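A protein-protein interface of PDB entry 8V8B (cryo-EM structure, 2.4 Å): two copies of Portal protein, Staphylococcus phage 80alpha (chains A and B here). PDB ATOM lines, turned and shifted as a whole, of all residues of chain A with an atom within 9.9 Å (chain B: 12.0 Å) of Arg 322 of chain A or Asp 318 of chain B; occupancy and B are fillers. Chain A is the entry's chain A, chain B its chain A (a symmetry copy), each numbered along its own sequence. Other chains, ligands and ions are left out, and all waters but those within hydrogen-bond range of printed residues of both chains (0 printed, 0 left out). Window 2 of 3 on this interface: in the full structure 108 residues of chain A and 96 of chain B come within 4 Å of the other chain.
Val 315 of chain A touches Tyr 316 of chain B, but with the chains exchanged Tyr 316 of chain A does not touch Val 315 of chain B (11.0 Å). Glu 320 of chain A touches Ala 319 of chain B, but with the chains exchanged Ala 319 of chain A does not touch Glu 320 of chain B (9.3 Å). Glu 323 of chain A touches Tyr 316 of chain B, but with the chains exchanged Tyr 316 of chain A does not touch Glu 323 of chain B (12.9 Å). Glu 325 of chain A touches Tyr 316 of chain B, but with the chains exchanged Tyr 316 of chain A does not touch Glu 325 of chain B (11.9 Å). Of the 6 pairs that touch across the chains among the printed residues, none has its exchanged pair printed and touching as well.
Arg 322 of chain A touches just one residue of chain B: Asp 318. Printed residues of chain A within 4 Å of Asp 318 of chain B: Arg 322 (3.8 Å). Val 317 of chain A touches none of the printed residues of chain B. No residue of chain B comes within 4 Å of Asp 318 of chain A. No residue of chain B comes within 4 Å of Gly 321 of chain A. Glu 323 of chain A touches one residue of chain B. No residue of chain B comes within 4 Å of Thr 324 of chain A. No residue of chain A comes within 4 Å of Gly 321 of chain B. No residue of chain A comes within 4 Å of Arg 322 of chain B. Printed residues of chain A within 4 Å of Tyr 316 of chain B: Val 315 (3.9 Å), Glu 323 (3.6 Å) and Glu 325 (2.8 Å). Of the printed residues of chain A, Gly 326 of chain B touches Glu 325. Of the printed residues of chain B, Glu 325 of chain A touches Tyr 316 and Gly 326. Printed residues of chain B within 4 Å of Val 315 of chain A: Tyr 316. Thr 314 of chain B touches none of the printed residues of chain A. Glu 323 of chain B touches none of the printed residues of chain A. The nearest residue of chain B that does not touch Arg 322 of chain A is Ala 319 of chain B (4.8 Å). The nearest residue of chain A that does not touch Asp 318 of chain B is Glu 323 of chain A (4.2 Å). The nearest printed residue of chain B that does not touch Val 315 of chain A is Thr 314 of chain B (6.3 Å).
OD2 of Asp 318 of chain B is in salt-bridge range of NH1 of Arg 322 of chain B (2.8 Å). O of Thr 324 of chain B lies within hydrogen-bond range of N of Tyr 316 of chain B, at 2.8 Å. The backbone carbonyl oxygen of Thr 314 of chain B is in hydrogen-bond range of the backbone NH of Gly 326 of chain B (2.9 Å). The guanidinium group (NH1) of Arg 322 of chain A lies within salt-bridge range of the side-chain carboxylate (OD2) of Asp 318 of chain A, at 2.8 Å. OH of Tyr 316 of chain B is in hydrogen-bond range of OG1 of Thr 314 of chain B, 3.4 Å away.
Of the 11 printed residues of chain A, 5 touch a printed residue of chain B. Hydrophobic or aromatic side chains of chain A within 4 Å of the printed part of chain B: Val 315. Along chain B the printed residues that touch a printed residue of chain A span positions 316 to 326. Among the printed residues, 6 pairs touch across the chains.
OE1 of Glu 325 of chain A is in hydrogen-bond range of OH of Tyr 316 of chain B, at 2.8 Å.
CG2 of Val 315 of chain A touches OH of Tyr 316 of chain B (3.9 Å). Glu 320 of chain A touches Ala 319 of chain B (O to CB, 3.3 Å). Arg 322 of chain A touches Asp 318 of chain B. OE1 of Glu 323 of chain A touches CD1 of Tyr 316 of chain B, 3.6 Å away. OE2 of Glu 325 of chain A touches CA of Gly 326 of chain B, at 3.8 Å.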
ATOM      1  N   VAL A 315      27.868 -20.155 -17.903  1.00  0.00           N
ATOM      2  CA  VAL A 315      27.877 -19.013 -18.814  1.00  0.00           C
ATOM      3  C   VAL A 315      27.658 -17.727 -18.023  1.00  0.00           C
ATOM      4  O   VAL A 315      26.704 -17.623 -17.242  1.00  0.00           O
ATOM      5  CB  VAL A 315      26.805 -19.167 -19.908  1.00  0.00           C
ATOM      6  CG1 VAL A 315      26.962 -18.079 -20.963  1.00  0.00           C
ATOM      7  CG2 VAL A 315      26.869 -20.554 -20.539  1.00  0.00           C
ATOM      8  N   TYR A 316      28.541 -16.752 -18.232  1.00  0.00           N
ATOM      9  CA  TYR A 316      28.474 -15.427 -17.630  1.00  0.00           C
ATOM     10  C   TYR A 316      27.886 -14.451 -18.645  1.00  0.00           C
ATOM     11  O   TYR A 316      28.245 -14.488 -19.825  1.00  0.00           O
ATOM     12  CB  TYR A 316      29.871 -14.961 -17.211  1.00  0.00           C
ATOM     13  CG  TYR A 316      30.593 -15.960 -16.337  1.00  0.00           C
ATOM     14  CD1 TYR A 316      30.049 -16.386 -15.134  1.00  0.00           C
ATOM     15  CD2 TYR A 316      31.806 -16.510 -16.738  1.00  0.00           C
ATOM     16  CE1 TYR A 316      30.703 -17.309 -14.344  1.00  0.00           C
ATOM     17  CE2 TYR A 316      32.466 -17.430 -15.956  1.00  0.00           C
ATOM     18  CZ  TYR A 316      31.912 -17.827 -14.763  1.00  0.00           C
ATOM     19  OH  TYR A 316      32.569 -18.752 -13.985  1.00  0.00           O
ATOM     20  N   VAL A 317      26.996 -13.566 -18.191  1.00  0.00           N
ATOM     21  CA  VAL A 317      26.315 -12.622 -19.078  1.00  0.00           C
ATOM     22  C   VAL A 317      26.595 -11.191 -18.622  1.00  0.00           C
ATOM     23  O   VAL A 317      26.333 -10.836 -17.466  1.00  0.00           O
ATOM     24  CB  VAL A 317      24.802 -12.890 -19.139  1.00  0.00           C
ATOM     25  CG1 VAL A 317      24.149 -12.635 -17.788  1.00  0.00           C
ATOM     26  CG2 VAL A 317      24.154 -12.026 -20.215  1.00  0.00           C
ATOM     27  N   ASP A 318      27.111 -10.374 -19.542  1.00  0.00           N
ATOM     28  CA  ASP A 318      27.398  -8.966 -19.285  1.00  0.00           C
ATOM     29  C   ASP A 318      26.116  -8.139 -19.180  1.00  0.00           C
ATOM     30  O   ASP A 318      25.026  -8.569 -19.570  1.00  0.00           O
ATOM     31  CB  ASP A 318      28.268  -8.378 -20.397  1.00  0.00           C
ATOM     32  CG  ASP A 318      29.633  -9.031 -20.482  1.00  0.00           C
ATOM     33  OD1 ASP A 318      29.965  -9.843 -19.594  1.00  0.00           O
ATOM     34  OD2 ASP A 318      30.375  -8.725 -21.436  1.00  0.00           O
ATOM     35  N   ALA A 319      26.264  -6.925 -18.640  1.00  0.00           N
ATOM     36  CA  ALA A 319      25.183  -5.947 -18.709  1.00  0.00           C
ATOM     37  C   ALA A 319      24.854  -5.571 -20.150  1.00  0.00           C
ATOM     38  O   ALA A 319      23.697  -5.265 -20.460  1.00  0.00           O
ATOM     39  CB  ALA A 319      25.551  -4.695 -17.912  1.00  0.00           C
ATOM     40  N   GLU A 320      25.845  -5.594 -21.043  1.00  0.00           N
ATOM     41  CA  GLU A 320      25.589  -5.476 -22.476  1.00  0.00           C
ATOM     42  C   GLU A 320      25.046  -6.763 -23.088  1.00  0.00           C
ATOM     43  O   GLU A 320      24.997  -6.875 -24.318  1.00  0.00           O
ATOM     44  CB  GLU A 320      26.860  -5.041 -23.216  1.00  0.00           C
ATOM     45  CG  GLU A 320      27.397  -3.684 -22.772  1.00  0.00           C
ATOM     46  CD  GLU A 320      28.423  -3.109 -23.736  1.00  0.00           C
ATOM     47  OE1 GLU A 320      28.241  -3.260 -24.963  1.00  0.00           O
ATOM     48  OE2 GLU A 320      29.399  -2.483 -23.268  1.00  0.00           O
ATOM     49  N   GLY A 321      24.639  -7.730 -22.265  1.00  0.00           N
ATOM     50  CA  GLY A 321      24.029  -8.954 -22.742  1.00  0.00           C
ATOM     51  C   GLY A 321      24.970  -9.959 -23.372  1.00  0.00           C
ATOM     52  O   GLY A 321      24.510 -11.036 -23.766  1.00  0.00           O
ATOM     53  N   ARG A 322      26.261  -9.656 -23.486  1.00  0.00           N
ATOM     54  CA  ARG A 322      27.211 -10.631 -24.008  1.00  0.00           C
ATOM     55  C   ARG A 322      27.274 -11.866 -23.117  1.00  0.00           C
ATOM     56  O   ARG A 322      27.335 -11.763 -21.890  1.00  0.00           O
ATOM     57  CB  ARG A 322      28.607 -10.020 -24.120  1.00  0.00           C
ATOM     58  CG  ARG A 322      28.714  -8.854 -25.073  1.00  0.00           C
ATOM     59  CD  ARG A 322      30.139  -8.335 -25.095  1.00  0.00           C
ATOM     60  NE  ARG A 322      31.069  -9.371 -25.537  1.00  0.00           N
ATOM     61  CZ  ARG A 322      31.896 -10.043 -24.743  1.00  0.00           C
ATOM     62  NH1 ARG A 322      31.948  -9.817 -23.439  1.00  0.00           N
ATOM     63  NH2 ARG A 322      32.687 -10.972 -25.271  1.00  0.00           N
ATOM     64  N   GLU A 323      27.279 -13.040 -23.744  1.00  0.00           N
ATOM     65  CA  GLU A 323      27.443 -14.308 -23.044  1.00  0.00           C
ATOM     66  C   GLU A 323      28.809 -14.906 -23.356  1.00  0.00           C
ATOM     67  O   GLU A 323      29.185 -15.030 -24.525  1.00  0.00           O
ATOM     68  CB  GLU A 323      26.333 -15.285 -23.430  1.00  0.00           C
ATOM     69  CG  GLU A 323      25.017 -14.969 -22.750  1.00  0.00           C
ATOM     70  CD  GLU A 323      23.927 -15.957 -23.092  1.00  0.00           C
ATOM     71  OE1 GLU A 323      24.126 -16.769 -24.019  1.00  0.00           O
ATOM     72  OE2 GLU A 323      22.867 -15.919 -22.432  1.00  0.00           O
ATOM     73  N   THR A 324      29.546 -15.269 -22.305  1.00  0.00           N
ATOM     74  CA  THR A 324      30.823 -15.967 -22.426  1.00  0.00           C
ATOM     75  C   THR A 324      30.860 -17.126 -21.440  1.00  0.00           C
ATOM     76  O   THR A 324      30.472 -16.965 -20.283  1.00  0.00           O
ATOM     77  CB  THR A 324      31.998 -15.016 -22.172  1.00  0.00           C
ATOM     78  OG1 THR A 324      31.854 -14.405 -20.884  1.00  0.00           O
ATOM     79  CG2 THR A 324      32.044 -13.931 -23.241  1.00  0.00           C
ATOM     80  N   GLU A 325      31.315 -18.292 -21.896  1.00  0.00           N
ATOM     81  CA  GLU A 325      31.474 -19.447 -21.017  1.00  0.00           C
ATOM     82  C   GLU A 325      32.793 -19.402 -20.246  1.00  0.00           C
ATOM     83  O   GLU A 325      33.797 -18.860 -20.715  1.00  0.00           O
ATOM     84  CB  GLU A 325      31.394 -20.746 -21.819  1.00  0.00           C
ATOM     85  CG  GLU A 325      32.514 -20.923 -22.836  1.00  0.00           C
ATOM     86  CD  GLU A 325      32.395 -22.216 -23.620  1.00  0.00           C
ATOM     87  OE1 GLU A 325      31.275 -22.753 -23.730  1.00  0.00           O
ATOM     88  OE2 GLU A 325      33.424 -22.692 -24.137  1.00  0.00           O
ATOM     89  N   THR B 314      27.411 -25.180 -28.399  1.00  0.00           N
ATOM     90  CA  THR B 314      26.341 -24.186 -28.387  1.00  0.00           C
ATOM     91  C   THR B 314      26.837 -22.838 -28.905  1.00  0.00           C
ATOM     92  O   THR B 314      28.014 -22.491 -28.776  1.00  0.00           O
ATOM     93  CB  THR B 314      25.775 -24.005 -26.982  1.00  0.00           C
ATOM     94  OG1 THR B 314      26.821 -23.604 -26.092  1.00  0.00           O
ATOM     95  CG2 THR B 314      25.148 -25.300 -26.486  1.00  0.00           C
ATOM     96  N   VAL B 315      25.915 -22.074 -29.489  1.00  0.00           N
ATOM     97  CA  VAL B 315      26.193 -20.740 -30.015  1.00  0.00           C
ATOM     98  C   VAL B 315      25.587 -19.689 -29.090  1.00  0.00           C
ATOM     99  O   VAL B 315      24.400 -19.758 -28.751  1.00  0.00           O
ATOM    100  CB  VAL B 315      25.647 -20.584 -31.446  1.00  0.00           C
ATOM    101  CG1 VAL B 315      26.121 -19.269 -32.056  1.00  0.00           C
ATOM    102  CG2 VAL B 315      26.055 -21.768 -32.316  1.00  0.00           C
ATOM    103  N   TYR B 316      26.407 -18.718 -28.690  1.00  0.00           N
ATOM    104  CA  TYR B 316      26.011 -17.586 -27.862  1.00  0.00           C
ATOM    105  C   TYR B 316      25.794 -16.370 -28.758  1.00  0.00           C
ATOM    106  O   TYR B 316      26.586 -16.119 -29.669  1.00  0.00           O
ATOM    107  CB  TYR B 316      27.094 -17.281 -26.825  1.00  0.00           C
ATOM    108  CG  TYR B 316      27.492 -18.487 -26.007  1.00  0.00           C
ATOM    109  CD1 TYR B 316      26.556 -19.187 -25.260  1.00  0.00           C
ATOM    110  CD2 TYR B 316      28.803 -18.953 -26.015  1.00  0.00           C
ATOM    111  CE1 TYR B 316      26.917 -20.297 -24.524  1.00  0.00           C
ATOM    112  CE2 TYR B 316      29.173 -20.058 -25.284  1.00  0.00           C
ATOM    113  CZ  TYR B 316      28.229 -20.727 -24.543  1.00  0.00           C
ATOM    114  OH  TYR B 316      28.597 -21.836 -23.818  1.00  0.00           O
ATOM    115  N   VAL B 317      24.734 -15.603 -28.493  1.00  0.00           N
ATOM    116  CA  VAL B 317      24.384 -14.448 -29.320  1.00  0.00           C
ATOM    117  C   VAL B 317      24.355 -13.186 -28.458  1.00  0.00           C
ATOM    118  O   VAL B 317      23.638 -13.127 -27.452  1.00  0.00           O
ATOM    119  CB  VAL B 317      23.039 -14.649 -30.038  1.00  0.00           C
ATOM    120  CG1 VAL B 317      21.893 -14.725 -29.038  1.00  0.00           C
ATOM    121  CG2 VAL B 317      22.799 -13.524 -31.038  1.00  0.00           C
ATOM    122  N   ASP B 318      25.127 -12.178 -28.871  1.00  0.00           N
ATOM    123  CA  ASP B 318      25.184 -10.889 -28.189  1.00  0.00           C
ATOM    124  C   ASP B 318      23.905 -10.080 -28.403  1.00  0.00           C
ATOM    125  O   ASP B 318      23.089 -10.367 -29.284  1.00  0.00           O
ATOM    126  CB  ASP B 318      26.372 -10.065 -28.686  1.00  0.00           C
ATOM    127  CG  ASP B 318      27.708 -10.713 -28.380  1.00  0.00           C
ATOM    128  OD1 ASP B 318      27.727 -11.732 -27.659  1.00  0.00           O
ATOM    129  OD2 ASP B 318      28.737 -10.198 -28.857  1.00  0.00           O
ATOM    130  N   ALA B 319      23.740  -9.046 -27.572  1.00  0.00           N
ATOM    131  CA  ALA B 319      22.700  -8.052 -27.825  1.00  0.00           C
ATOM    132  C   ALA B 319      22.932  -7.316 -29.140  1.00  0.00           C
ATOM    133  O   ALA B 319      21.968  -6.910 -29.798  1.00  0.00           O
ATOM    134  CB  ALA B 319      22.634  -7.052 -26.669  1.00  0.00           C
ATOM    135  N   GLU B 320      24.192  -7.141 -29.544  1.00  0.00           N
ATOM    136  CA  GLU B 320      24.506  -6.658 -30.886  1.00  0.00           C
ATOM    137  C   GLU B 320      24.343  -7.734 -31.955  1.00  0.00           C
ATOM    138  O   GLU B 320      24.786  -7.531 -33.091  1.00  0.00           O
ATOM    139  CB  GLU B 320      25.929  -6.087 -30.933  1.00  0.00           C
ATOM    140  CG  GLU B 320      26.147  -4.902 -29.999  1.00  0.00           C
ATOM    141  CD  GLU B 320      27.422  -4.131 -30.306  1.00  0.00           C
ATOM    142  OE1 GLU B 320      27.744  -3.963 -31.502  1.00  0.00           O
ATOM    143  OE2 GLU B 320      28.088  -3.670 -29.354  1.00  0.00           O
ATOM    144  N   GLY B 321      23.721  -8.865 -31.622  1.00  0.00           N
ATOM    145  CA  GLY B 321      23.439  -9.912 -32.582  1.00  0.00           C
ATOM    146  C   GLY B 321      24.623 -10.752 -33.012  1.00  0.00           C
ATOM    147  O   GLY B 321      24.436 -11.681 -33.803  1.00  0.00           O
ATOM    148  N   ARG B 322      25.830 -10.465 -32.527  1.00  0.00           N
ATOM    149  CA  ARG B 322      26.979 -11.305 -32.850  1.00  0.00           C
ATOM    150  C   ARG B 322      26.781 -12.725 -32.334  1.00  0.00           C
ATOM    151  O   ARG B 322      26.352 -12.936 -31.198  1.00  0.00           O
ATOM    152  CB  ARG B 322      28.257 -10.725 -32.248  1.00  0.00           C
ATOM    153  CG  ARG B 322      28.641  -9.359 -32.767  1.00  0.00           C
ATOM    154  CD  ARG B 322      29.918  -8.892 -32.096  1.00  0.00           C
ATOM    155  NE  ARG B 322      31.021  -9.809 -32.371  1.00  0.00           N
ATOM    156  CZ  ARG B 322      31.521 -10.682 -31.503  1.00  0.00           C
ATOM    157  NH1 ARG B 322      31.044 -10.793 -30.273  1.00  0.00           N
ATOM    158  NH2 ARG B 322      32.522 -11.469 -31.882  1.00  0.00           N
ATOM    159  N   GLU B 323      27.119 -13.703 -33.172  1.00  0.00           N
ATOM    160  CA  GLU B 323      27.091 -15.111 -32.795  1.00  0.00           C
ATOM    161  C   GLU B 323      28.511 -15.649 -32.674  1.00  0.00           C
ATOM    162  O   GLU B 323      29.322 -15.485 -33.591  1.00  0.00           O
ATOM    163  CB  GLU B 323      26.296 -15.927 -33.813  1.00  0.00           C
ATOM    164  CG  GLU B 323      24.800 -15.756 -33.655  1.00  0.00           C
ATOM    165  CD  GLU B 323      24.007 -16.595 -34.628  1.00  0.00           C
ATOM    166  OE1 GLU B 323      24.611 -17.152 -35.568  1.00  0.00           O
ATOM    167  OE2 GLU B 323      22.773 -16.694 -34.455  1.00  0.00           O
ATOM    168  N   THR B 324      28.805 -16.285 -31.540  1.00  0.00           N
ATOM    169  CA  THR B 324      30.077 -16.966 -31.311  1.00  0.00           C
ATOM    170  C   THR B 324      29.813 -18.337 -30.703  1.00  0.00           C
ATOM    171  O   THR B 324      28.994 -18.461 -29.792  1.00  0.00           O
ATOM    172  CB  THR B 324      30.985 -16.144 -30.390  1.00  0.00           C
ATOM    173  OG1 THR B 324      30.305 -15.872 -29.159  1.00  0.00           O
ATOM    174  CG2 THR B 324      31.362 -14.826 -31.056  1.00  0.00           C
ATOM    175  N   GLU B 325      30.496 -19.362 -31.209  1.00  0.00           N
ATOM    176  CA  GLU B 325      30.386 -20.705 -30.647  1.00  0.00           C
ATOM    177  C   GLU B 325      31.292 -20.893 -29.432  1.00  0.00           C
ATOM    178  O   GLU B 325      32.357 -20.280 -29.319  1.00  0.00           O
ATOM    179  CB  GLU B 325      30.722 -21.758 -31.705  1.00  0.00           C
ATOM    180  CG  GLU B 325      32.160 -21.704 -32.205  1.00  0.00           C
ATOM    181  CD  GLU B 325      32.454 -22.754 -33.260  1.00  0.00           C
ATOM    182  OE1 GLU B 325      31.508 -23.214 -33.930  1.00  0.00           O
ATOM    183  OE2 GLU B 325      33.635 -23.113 -33.425  1.00  0.00           O
ATOM    184  N   GLY B 326      30.845 -21.756 -28.514  1.00  0.00           N
ATOM    185  CA  GLY B 326      31.686 -22.238 -27.429  1.00  0.00           C
ATOM    186  C   GLY B 326      32.776 -23.210 -27.869  1.00  0.00           C
ATOM    187  O   GLY B 326      32.838 -23.673 -29.008  1.00  0.00           O
